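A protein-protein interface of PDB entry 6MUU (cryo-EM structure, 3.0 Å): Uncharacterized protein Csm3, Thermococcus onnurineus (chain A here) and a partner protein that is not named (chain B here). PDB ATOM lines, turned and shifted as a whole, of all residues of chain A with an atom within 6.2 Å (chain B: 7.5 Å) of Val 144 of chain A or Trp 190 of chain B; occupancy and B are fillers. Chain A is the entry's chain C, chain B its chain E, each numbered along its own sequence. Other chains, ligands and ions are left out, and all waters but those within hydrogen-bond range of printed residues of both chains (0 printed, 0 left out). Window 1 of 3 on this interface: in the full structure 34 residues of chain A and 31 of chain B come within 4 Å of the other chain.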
ATOM      1  N   PRO A  52      27.847   2.948 -10.517  1.00  0.00           N
ATOM      2  CA  PRO A  52      26.722   3.734 -11.022  1.00  0.00           C
ATOM      3  C   PRO A  52      26.859   5.210 -10.694  1.00  0.00           C
ATOM      4  O   PRO A  52      27.608   5.615  -9.807  1.00  0.00           O
ATOM      5  CB  PRO A  52      25.518   3.131 -10.302  1.00  0.00           C
ATOM      6  CG  PRO A  52      25.943   1.807  -9.907  1.00  0.00           C
ATOM      7  CD  PRO A  52      27.386   1.908  -9.589  1.00  0.00           C
ATOM      8  N   GLY A  53      26.117   6.025 -11.436  1.00  0.00           N
ATOM      9  CA  GLY A  53      26.042   7.426 -11.090  1.00  0.00           C
ATOM     10  C   GLY A  53      25.222   7.683  -9.855  1.00  0.00           C
ATOM     11  O   GLY A  53      25.424   8.697  -9.189  1.00  0.00           O
ATOM     12  N   SER A  54      24.301   6.778  -9.540  1.00  0.00           N
ATOM     13  CA  SER A  54      23.474   6.912  -8.350  1.00  0.00           C
ATOM     14  C   SER A  54      24.267   6.637  -7.087  1.00  0.00           C
ATOM     15  O   SER A  54      24.033   7.275  -6.058  1.00  0.00           O
ATOM     16  CB  SER A  54      22.291   5.967  -8.460  1.00  0.00           C
ATOM     17  OG  SER A  54      22.753   4.650  -8.658  1.00  0.00           O
ATOM     18  N   LEU A  56      27.564   7.107  -6.689  1.00  0.00           N
ATOM     19  CA  LEU A  56      28.571   8.126  -6.432  1.00  0.00           C
ATOM     20  C   LEU A  56      27.932   9.452  -6.059  1.00  0.00           C
ATOM     21  O   LEU A  56      28.429  10.139  -5.173  1.00  0.00           O
ATOM     22  CB  LEU A  56      29.495   8.277  -7.637  1.00  0.00           C
ATOM     23  CG  LEU A  56      30.690   9.208  -7.434  1.00  0.00           C
ATOM     24  CD1 LEU A  56      31.501   8.739  -6.259  1.00  0.00           C
ATOM     25  CD2 LEU A  56      31.552   9.224  -8.664  1.00  0.00           C
ATOM     26  N   LYS A  57      26.827   9.822  -6.706  1.00  0.00           N
ATOM     27  CA  LYS A  57      26.117  11.036  -6.320  1.00  0.00           C
ATOM     28  C   LYS A  57      25.461  10.879  -4.962  1.00  0.00           C
ATOM     29  O   LYS A  57      25.491  11.799  -4.136  1.00  0.00           O
ATOM     30  CB  LYS A  57      25.062  11.388  -7.360  1.00  0.00           C
ATOM     31  CG  LYS A  57      24.313  12.642  -7.015  1.00  0.00           C
ATOM     32  CD  LYS A  57      23.224  12.966  -7.978  1.00  0.00           C
ATOM     33  CE  LYS A  57      22.508  14.202  -7.505  1.00  0.00           C
ATOM     34  NZ  LYS A  57      21.415  14.622  -8.397  1.00  0.00           N
ATOM     35  N   LEU A  60      28.187  11.180  -2.282  1.00  0.00           N
ATOM     36  CA  LEU A  60      28.645  12.554  -2.124  1.00  0.00           C
ATOM     37  C   LEU A  60      27.582  13.438  -1.494  1.00  0.00           C
ATOM     38  O   LEU A  60      27.922  14.387  -0.787  1.00  0.00           O
ATOM     39  CB  LEU A  60      29.050  13.154  -3.466  1.00  0.00           C
ATOM     40  CG  LEU A  60      30.232  12.648  -4.282  1.00  0.00           C
ATOM     41  CD1 LEU A  60      30.304  13.409  -5.586  1.00  0.00           C
ATOM     42  CD2 LEU A  60      31.517  12.742  -3.536  1.00  0.00           C
ATOM     43  N   PHE A 129      22.709  19.573  -5.540  1.00  0.00           N
ATOM     44  CA  PHE A 129      22.191  18.241  -5.784  1.00  0.00           C
ATOM     45  C   PHE A 129      20.731  18.225  -6.200  1.00  0.00           C
ATOM     46  O   PHE A 129      20.298  17.261  -6.836  1.00  0.00           O
ATOM     47  CB  PHE A 129      22.383  17.386  -4.540  1.00  0.00           C
ATOM     48  CG  PHE A 129      23.813  17.072  -4.247  1.00  0.00           C
ATOM     49  CD1 PHE A 129      24.461  16.062  -4.926  1.00  0.00           C
ATOM     50  CD2 PHE A 129      24.513  17.777  -3.290  1.00  0.00           C
ATOM     51  CE1 PHE A 129      25.774  15.766  -4.655  1.00  0.00           C
ATOM     52  CE2 PHE A 129      25.827  17.484  -3.024  1.00  0.00           C
ATOM     53  CZ  PHE A 129      26.454  16.480  -3.709  1.00  0.00           C
ATOM     54  N   ILE A 142      24.750  19.200 -11.052  1.00  0.00           N
ATOM     55  CA  ILE A 142      25.788  18.248 -11.412  1.00  0.00           C
ATOM     56  C   ILE A 142      25.166  17.060 -12.123  1.00  0.00           C
ATOM     57  O   ILE A 142      23.998  16.722 -11.923  1.00  0.00           O
ATOM     58  CB  ILE A 142      26.616  17.784 -10.200  1.00  0.00           C
ATOM     59  CG1 ILE A 142      25.745  17.101  -9.161  1.00  0.00           C
ATOM     60  CG2 ILE A 142      27.352  18.941  -9.604  1.00  0.00           C
ATOM     61  CD1 ILE A 142      26.552  16.341  -8.164  1.00  0.00           C
ATOM     62  N   ILE A 143      25.962  16.432 -12.980  1.00  0.00           N
ATOM     63  CA  ILE A 143      25.651  15.141 -13.570  1.00  0.00           C
ATOM     64  C   ILE A 143      26.804  14.215 -13.242  1.00  0.00           C
ATOM     65  O   ILE A 143      27.935  14.456 -13.672  1.00  0.00           O
ATOM     66  CB  ILE A 143      25.444  15.230 -15.087  1.00  0.00           C
ATOM     67  CG1 ILE A 143      24.178  16.007 -15.419  1.00  0.00           C
ATOM     68  CG2 ILE A 143      25.421  13.856 -15.694  1.00  0.00           C
ATOM     69  CD1 ILE A 143      24.033  16.292 -16.874  1.00  0.00           C
ATOM     70  N   VAL A 144      26.535  13.175 -12.470  1.00  0.00           N
ATOM     71  CA  VAL A 144      27.555  12.204 -12.114  1.00  0.00           C
ATOM     72  C   VAL A 144      27.352  11.012 -13.035  1.00  0.00           C
ATOM     73  O   VAL A 144      26.471  10.185 -12.817  1.00  0.00           O
ATOM     74  CB  VAL A 144      27.490  11.813 -10.640  1.00  0.00           C
ATOM     75  CG1 VAL A 144      28.606  10.860 -10.311  1.00  0.00           C
ATOM     76  CG2 VAL A 144      27.586  13.042  -9.775  1.00  0.00           C
ATOM     77  N   ARG A 145      28.161  10.949 -14.082  1.00  0.00           N
ATOM     78  CA  ARG A 145      28.123   9.862 -15.045  1.00  0.00           C
ATOM     79  C   ARG A 145      28.620   8.572 -14.396  1.00  0.00           C
ATOM     80  O   ARG A 145      29.387   8.601 -13.433  1.00  0.00           O
ATOM     81  CB  ARG A 145      28.983  10.253 -16.248  1.00  0.00           C
ATOM     82  CG  ARG A 145      29.049   9.302 -17.417  1.00  0.00           C
ATOM     83  CD  ARG A 145      30.053   9.813 -18.412  1.00  0.00           C
ATOM     84  NE  ARG A 145      30.415   8.802 -19.395  1.00  0.00           N
ATOM     85  CZ  ARG A 145      31.349   8.981 -20.320  1.00  0.00           C
ATOM     86  NH1 ARG A 145      31.627   8.014 -21.182  1.00  0.00           N
ATOM     87  NH2 ARG A 145      32.007  10.130 -20.377  1.00  0.00           N
ATOM     88  N   ASP A 146      28.146   7.435 -14.913  1.00  0.00           N
ATOM     89  CA  ASP A 146      28.656   6.128 -14.512  1.00  0.00           C
ATOM     90  C   ASP A 146      30.148   6.010 -14.805  1.00  0.00           C
ATOM     91  O   ASP A 146      30.686   6.675 -15.691  1.00  0.00           O
ATOM     92  CB  ASP A 146      27.917   5.017 -15.250  1.00  0.00           C
ATOM     93  CG  ASP A 146      26.453   4.975 -14.920  1.00  0.00           C
ATOM     94  OD1 ASP A 146      26.080   5.436 -13.828  1.00  0.00           O
ATOM     95  OD2 ASP A 146      25.672   4.466 -15.745  1.00  0.00           O
ATOM     96  N   GLU A 196      33.269  11.028 -14.490  1.00  0.00           N
ATOM     97  CA  GLU A 196      33.060  12.351 -15.052  1.00  0.00           C
ATOM     98  C   GLU A 196      31.953  13.037 -14.271  1.00  0.00           C
ATOM     99  O   GLU A 196      30.923  12.424 -13.996  1.00  0.00           O
ATOM    100  CB  GLU A 196      32.679  12.281 -16.529  1.00  0.00           C
ATOM    101  CG  GLU A 196      32.474  13.624 -17.170  1.00  0.00           C
ATOM    102  CD  GLU A 196      32.099  13.515 -18.623  1.00  0.00           C
ATOM    103  OE1 GLU A 196      32.009  12.380 -19.134  1.00  0.00           O
ATOM    104  OE2 GLU A 196      31.883  14.567 -19.256  1.00  0.00           O
ATOM    105  N   ILE A 197      32.162  14.301 -13.912  1.00  0.00           N
ATOM    106  CA  ILE A 197      31.123  15.116 -13.294  1.00  0.00           C
ATOM    107  C   ILE A 197      30.948  16.378 -14.127  1.00  0.00           C
ATOM    108  O   ILE A 197      31.913  17.107 -14.362  1.00  0.00           O
ATOM    109  CB  ILE A 197      31.442  15.467 -11.833  1.00  0.00           C
ATOM    110  CG1 ILE A 197      31.535  14.200 -10.993  1.00  0.00           C
ATOM    111  CG2 ILE A 197      30.354  16.314 -11.254  1.00  0.00           C
ATOM    112  CD1 ILE A 197      32.082  14.424  -9.627  1.00  0.00           C
ATOM    113  N   ILE A 198      29.726  16.629 -14.579  1.00  0.00           N
ATOM    114  CA  ILE A 198      29.400  17.795 -15.391  1.00  0.00           C
ATOM    115  C   ILE A 198      28.596  18.746 -14.524  1.00  0.00           C
ATOM    116  O   ILE A 198      27.451  18.450 -14.178  1.00  0.00           O
ATOM    117  CB  ILE A 198      28.606  17.411 -16.646  1.00  0.00           C
ATOM    118  CG1 ILE A 198      29.401  16.436 -17.501  1.00  0.00           C
ATOM    119  CG2 ILE A 198      28.268  18.641 -17.449  1.00  0.00           C
ATOM    120  CD1 ILE A 198      28.598  15.798 -18.585  1.00  0.00           C
ATOM    121  N   LEU A 214      31.586  20.568  -3.990  1.00  0.00           N
ATOM    122  CA  LEU A 214      31.694  19.277  -4.652  1.00  0.00           C
ATOM    123  C   LEU A 214      33.047  18.638  -4.386  1.00  0.00           C
ATOM    124  O   LEU A 214      33.135  17.423  -4.203  1.00  0.00           O
ATOM    125  CB  LEU A 214      31.455  19.445  -6.146  1.00  0.00           C
ATOM    126  CG  LEU A 214      31.473  18.172  -6.980  1.00  0.00           C
ATOM    127  CD1 LEU A 214      30.353  17.252  -6.561  1.00  0.00           C
ATOM    128  CD2 LEU A 214      31.374  18.529  -8.439  1.00  0.00           C
ATOM    129  N   GLY B  13      26.089   5.902 -21.773  1.00  0.00           N
ATOM    130  CA  GLY B  13      25.600   5.101 -20.680  1.00  0.00           C
ATOM    131  C   GLY B  13      24.232   4.529 -20.983  1.00  0.00           C
ATOM    132  O   GLY B  13      23.953   4.103 -22.106  1.00  0.00           O
ATOM    133  N   PRO B  14      23.353   4.497 -19.990  1.00  0.00           N
ATOM    134  CA  PRO B  14      21.983   4.051 -20.232  1.00  0.00           C
ATOM    135  C   PRO B  14      21.097   5.188 -20.715  1.00  0.00           C
ATOM    136  O   PRO B  14      21.395   6.363 -20.534  1.00  0.00           O
ATOM    137  CB  PRO B  14      21.532   3.574 -18.850  1.00  0.00           C
ATOM    138  CG  PRO B  14      22.293   4.412 -17.922  1.00  0.00           C
ATOM    139  CD  PRO B  14      23.626   4.660 -18.554  1.00  0.00           C
ATOM    140  N   VAL B 129      17.133  -2.146 -12.750  1.00  0.00           N
ATOM    141  CA  VAL B 129      18.194  -1.888 -11.785  1.00  0.00           C
ATOM    142  C   VAL B 129      17.556  -1.416 -10.482  1.00  0.00           C
ATOM    143  O   VAL B 129      16.811  -0.425 -10.493  1.00  0.00           O
ATOM    144  CB  VAL B 129      19.223  -0.885 -12.331  1.00  0.00           C
ATOM    145  CG1 VAL B 129      20.099  -1.569 -13.345  1.00  0.00           C
ATOM    146  CG2 VAL B 129      18.556   0.285 -13.039  1.00  0.00           C
ATOM    147  N   ARG B 131      17.592   0.488  -6.994  1.00  0.00           N
ATOM    148  CA  ARG B 131      18.290   1.551  -6.307  1.00  0.00           C
ATOM    149  C   ARG B 131      17.925   1.464  -4.839  1.00  0.00           C
ATOM    150  O   ARG B 131      17.151   0.605  -4.431  1.00  0.00           O
ATOM    151  CB  ARG B 131      17.905   2.901  -6.888  1.00  0.00           C
ATOM    152  CG  ARG B 131      18.203   3.091  -8.349  1.00  0.00           C
ATOM    153  CD  ARG B 131      19.657   3.319  -8.590  1.00  0.00           C
ATOM    154  NE  ARG B 131      19.900   3.709  -9.968  1.00  0.00           N
ATOM    155  CZ  ARG B 131      20.338   2.892 -10.911  1.00  0.00           C
ATOM    156  NH1 ARG B 131      20.519   3.340 -12.141  1.00  0.00           N
ATOM    157  NH2 ARG B 131      20.640   1.643 -10.611  1.00  0.00           N
ATOM    158  N   VAL B 132      18.463   2.362  -4.025  1.00  0.00           N
ATOM    159  CA  VAL B 132      18.123   2.352  -2.612  1.00  0.00           C
ATOM    160  C   VAL B 132      18.021   3.793  -2.134  1.00  0.00           C
ATOM    161  O   VAL B 132      18.518   4.718  -2.770  1.00  0.00           O
ATOM    162  CB  VAL B 132      19.149   1.543  -1.780  1.00  0.00           C
ATOM    163  CG1 VAL B 132      20.321   2.369  -1.369  1.00  0.00           C
ATOM    164  CG2 VAL B 132      18.507   0.894  -0.612  1.00  0.00           C
ATOM    165  N   TYR B 144      13.667   0.751  -4.402  1.00  0.00           N
ATOM    166  CA  TYR B 144      12.689   0.973  -5.445  1.00  0.00           C
ATOM    167  C   TYR B 144      13.303   0.457  -6.731  1.00  0.00           C
ATOM    168  O   TYR B 144      14.507   0.221  -6.807  1.00  0.00           O
ATOM    169  CB  TYR B 144      12.290   2.449  -5.544  1.00  0.00           C
ATOM    170  CG  TYR B 144      13.427   3.409  -5.791  1.00  0.00           C
ATOM    171  CD1 TYR B 144      14.140   3.945  -4.736  1.00  0.00           C
ATOM    172  CD2 TYR B 144      13.760   3.818  -7.076  1.00  0.00           C
ATOM    173  CE1 TYR B 144      15.170   4.822  -4.952  1.00  0.00           C
ATOM    174  CE2 TYR B 144      14.789   4.708  -7.295  1.00  0.00           C
ATOM    175  CZ  TYR B 144      15.481   5.210  -6.225  1.00  0.00           C
ATOM    176  OH  TYR B 144      16.515   6.084  -6.423  1.00  0.00           O
ATOM    177  N   TRP B 146      13.889   0.559 -10.971  1.00  0.00           N
ATOM    178  CA  TRP B 146      14.119   1.557 -11.994  1.00  0.00           C
ATOM    179  C   TRP B 146      14.457   0.880 -13.314  1.00  0.00           C
ATOM    180  O   TRP B 146      15.205  -0.098 -13.342  1.00  0.00           O
ATOM    181  CB  TRP B 146      15.237   2.498 -11.568  1.00  0.00           C
ATOM    182  CG  TRP B 146      15.346   3.616 -12.479  1.00  0.00           C
ATOM    183  CD1 TRP B 146      16.267   3.791 -13.456  1.00  0.00           C
ATOM    184  CD2 TRP B 146      14.460   4.726 -12.553  1.00  0.00           C
ATOM    185  NE1 TRP B 146      16.024   4.958 -14.127  1.00  0.00           N
ATOM    186  CE2 TRP B 146      14.911   5.546 -13.591  1.00  0.00           C
ATOM    187  CE3 TRP B 146      13.325   5.106 -11.838  1.00  0.00           C
ATOM    188  CZ2 TRP B 146      14.265   6.715 -13.939  1.00  0.00           C
ATOM    189  CZ3 TRP B 146      12.695   6.275 -12.175  1.00  0.00           C
ATOM    190  CH2 TRP B 146      13.167   7.068 -13.213  1.00  0.00           C
ATOM    191  N   GLU B 148      15.936   0.977 -17.288  1.00  0.00           N
ATOM    192  CA  GLU B 148      16.908   1.632 -18.150  1.00  0.00           C
ATOM    193  C   GLU B 148      17.082   0.827 -19.427  1.00  0.00           C
ATOM    194  O   GLU B 148      16.913  -0.390 -19.443  1.00  0.00           O
ATOM    195  CB  GLU B 148      18.280   1.780 -17.478  1.00  0.00           C
ATOM    196  CG  GLU B 148      18.364   2.752 -16.313  1.00  0.00           C
ATOM    197  CD  GLU B 148      18.180   4.197 -16.729  1.00  0.00           C
ATOM    198  OE1 GLU B 148      18.551   4.540 -17.866  1.00  0.00           O
ATOM    199  OE2 GLU B 148      17.677   5.003 -15.920  1.00  0.00           O
ATOM    200  N   GLY B 186      14.790  11.538 -19.069  1.00  0.00           N
ATOM    201  CA  GLY B 186      15.100  10.501 -18.069  1.00  0.00           C
ATOM    202  C   GLY B 186      15.932  11.058 -16.935  1.00  0.00           C
ATOM    203  O   GLY B 186      16.146  12.273 -16.918  1.00  0.00           O
ATOM    204  N   LYS B 187      16.377  10.203 -16.023  1.00  0.00           N
ATOM    205  CA  LYS B 187      17.213  10.613 -14.865  1.00  0.00           C
ATOM    206  C   LYS B 187      18.579  11.061 -15.383  1.00  0.00           C
ATOM    207  O   LYS B 187      19.514  10.266 -15.286  1.00  0.00           O
ATOM    208  CB  LYS B 187      17.398   9.425 -13.919  1.00  0.00           C
ATOM    209  CG  LYS B 187      16.324   9.266 -12.856  1.00  0.00           C
ATOM    210  CD  LYS B 187      16.507  10.214 -11.701  1.00  0.00           C
ATOM    211  CE  LYS B 187      15.752   9.784 -10.465  1.00  0.00           C
ATOM    212  NZ  LYS B 187      14.335  10.209 -10.525  1.00  0.00           N
ATOM    213  N   SER B 188      18.717  12.306 -15.821  1.00  0.00           N
ATOM    214  CA  SER B 188      19.990  12.817 -16.397  1.00  0.00           C
ATOM    215  C   SER B 188      21.000  13.204 -15.311  1.00  0.00           C
ATOM    216  O   SER B 188      22.130  13.532 -15.676  1.00  0.00           O
ATOM    217  CB  SER B 188      19.736  13.962 -17.331  1.00  0.00           C
ATOM    218  OG  SER B 188      19.930  15.198 -16.667  1.00  0.00           O
ATOM    219  N   THR B 189      20.627  13.163 -14.039  1.00  0.00           N
ATOM    220  CA  THR B 189      21.536  13.487 -12.912  1.00  0.00           C
ATOM    221  C   THR B 189      22.398  12.260 -12.595  1.00  0.00           C
ATOM    222  O   THR B 189      23.388  12.421 -11.869  1.00  0.00           O
ATOM    223  CB  THR B 189      20.722  13.936 -11.696  1.00  0.00           C
ATOM    224  OG1 THR B 189      21.625  14.519 -10.762  1.00  0.00           O
ATOM    225  CG2 THR B 189      19.959  12.804 -11.047  1.00  0.00           C
ATOM    226  N   TRP B 190      22.026  11.085 -13.093  1.00  0.00           N
ATOM    227  CA  TRP B 190      22.798   9.832 -12.890  1.00  0.00           C
ATOM    228  C   TRP B 190      23.592   9.529 -14.162  1.00  0.00           C
ATOM    229  O   TRP B 190      24.099   8.412 -14.268  1.00  0.00           O
ATOM    230  CB  TRP B 190      21.861   8.665 -12.572  1.00  0.00           C
ATOM    231  CG  TRP B 190      21.142   8.782 -11.267  1.00  0.00           C
ATOM    232  CD1 TRP B 190      21.398   9.663 -10.259  1.00  0.00           C
ATOM    233  CD2 TRP B 190      20.038   7.977 -10.825  1.00  0.00           C
ATOM    234  NE1 TRP B 190      20.526   9.466  -9.225  1.00  0.00           N
ATOM    235  CE2 TRP B 190      19.681   8.438  -9.543  1.00  0.00           C
ATOM    236  CE3 TRP B 190      19.314   6.923 -11.388  1.00  0.00           C
ATOM    237  CZ2 TRP B 190      18.638   7.871  -8.815  1.00  0.00           C
ATOM    238  CZ3 TRP B 190      18.284   6.365 -10.668  1.00  0.00           C
ATOM    239  CH2 TRP B 190      17.951   6.836  -9.401  1.00  0.00           C
ATOM    240  N   GLY B 191      23.656  10.459 -15.102  1.00  0.00           N
ATOM    241  CA  GLY B 191      24.414  10.235 -16.345  1.00  0.00           C
ATOM    242  C   GLY B 191      23.607   9.494 -17.393  1.00  0.00           C
ATOM    243  O   GLY B 191      24.224   8.958 -18.327  1.00  0.00           O
ATOM    244  N   ALA B 192      22.290   9.465 -17.273  1.00  0.00           N
ATOM    245  CA  ALA B 192      21.445   8.763 -18.266  1.00  0.00           C
ATOM    246  C   ALA B 192      21.001   9.751 -19.349  1.00  0.00           C
ATOM    247  O   ALA B 192      20.541  10.841 -18.985  1.00  0.00           O
ATOM    248  CB  ALA B 192      20.263   8.133 -17.577  1.00  0.00           C
ATOM    249  N   GLY B 193      21.152   9.409 -20.621  1.00  0.00           N
ATOM    250  CA  GLY B 193      20.727  10.311 -21.707  1.00  0.00           C
ATOM    251  C   GLY B 193      21.884  11.102 -22.284  1.00  0.00           C
ATOM    252  O   GLY B 193      21.652  11.837 -23.254  1.00  0.00           O
ATOM    253  N   LEU B 194      23.075  10.987 -21.717  1.00  0.00           N
ATOM    254  CA  LEU B 194      24.255  11.727 -22.237  1.00  0.00           C
ATOM    255  C   LEU B 194      24.800  10.956 -23.440  1.00  0.00           C
ATOM    256  O   LEU B 194      24.720   9.722 -23.407  1.00  0.00           O
ATOM    257  CB  LEU B 194      25.299  11.833 -21.125  1.00  0.00           C
ATOM    258  CG  LEU B 194      24.824  12.525 -19.851  1.00  0.00           C
ATOM    259  CD1 LEU B 194      25.998  12.839 -18.944  1.00  0.00           C
ATOM    260  CD2 LEU B 194      24.068  13.796 -20.184  1.00  0.00           C
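The side-chain hydroxyl (OG) of Ser 54 of chain A lies within hydrogen-bond range of the guanidinium group (NE) of Arg 131 of chain B, 3.3 Å away.
The side-chain hydroxyl (OG1) of Thr 189 of chain B lies within hydrogen-bond range of the backbone carbonyl oxygen (O) of Ile 142 of chain A.
N of Val 144 of chain A is in hydrogen-bond range of O of Thr 189 of chain B, 3.3 Å away.
The side-chain amino group (NZ) of Lys 57 of chain A lies close to the side-chain hydroxyl (OG1) of Thr 189 of chain B.
The backbone carbonyl oxygen (O) of Val 144 of chain A sits close to the backbone carbonyl oxygen (O) of Trp 190 of chain B (3.3 Å).
The side-chain carboxylate of Asp 146 of chain A is in hydrogen-bond range of the backbone NH of Gly 53 of chain A (2.5 Å).
The side-chain amino group of Lys 57 of chain A sits at hydrogen-bond distance from the backbone carbonyl oxygen of Phe 129 of chain A (3.3 Å).
The backbone carbonyl oxygen of Ile 198 of chain A lies within hydrogen-bond range of the backbone NH of Ile 143 of chain A.
OE1 of Glu 196 of chain A lies within salt-bridge range of NH2 of Arg 145 of chain A (2.6 Å).
The backbone carbonyl oxygen of Pro 14 of chain B is in hydrogen-bond range of the backbone NH of Gly 193 of chain B.
N of Arg 131 of chain B is in hydrogen-bond range of O of Tyr 144 of chain B, 3.1 Å away.
Among the printed residues, merely in contact across the chains: Ile 143 of chain A with Ser 188 of chain B (3.2 Å), Ile 143 of chain A with Leu 194 of chain B (3.5 Å), Asp 146 of chain A with Pro 14 of chain B (3.5 Å), Asp 146 of chain A with Trp 190 of chain B (3.6 Å), Val 144 of chain A with Gly 191 of chain B (3.6 Å), Ser 54 of chain A with Trp 190 of chain B (3.8 Å), Ile 143 of chain A with Gly 191 of chain B (3.8 Å), Gly 53 of chain A with Trp 190 of chain B (3.9 Å), Ile 143 of chain A with Thr 189 of chain B (3.9 Å), Arg 145 of chain A with Gly 191 of chain B (3.9 Å) and Ile 198 of chain A with Leu 194 of chain B (3.96 Å).
Of the printed residues of chain B, Ser 54 of chain A touches Arg 131 and Trp 190.
Printed residues of chain B within 4 Å of Ile 142 of chain A: Thr 189.
Of the printed residues of chain B, Ile 143 of chain A touches Ser 188 (3.2 Å), Thr 189 (3.9 Å), Gly 191 (3.8 Å) and Leu 194 (3.5 Å).
Val 144 of chain A touches three residues of chain B.
Gly 186 of chain B touches none of the printed residues of chain A.
Lys 187 of chain B touches none of the printed residues of chain A.
Of chain A, only Gly 53, Ser 54, Val 144 and Asp 146 come within 4 Å of Trp 190 of chain B.
The nearest residue of chain B that does not touch Val 144 of chain A is Ser 188 of chain B (5.5 Å).
The nearest residue of chain A that does not touch Trp 190 of chain B is Arg 145 of chain A (4.3 Å).
Printed residues of chain A that touch a printed residue of chain B: Gly 53, Ser 54, Lys 57, Ile 142, Ile 143, Val 144, Arg 145, Asp 146 and Ile 198.
Of the 17 printed residues of chain B, 7 touch a printed residue of chain A.
Hydrophobic or aromatic side chains of chain B that line the printed part of chain A: Pro 14, Trp 190 and Leu 194.
Among the printed residues, no Asp or Glu carboxylate lies within 4 Å of a Lys or Arg side-chain nitrogen of the other chain.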
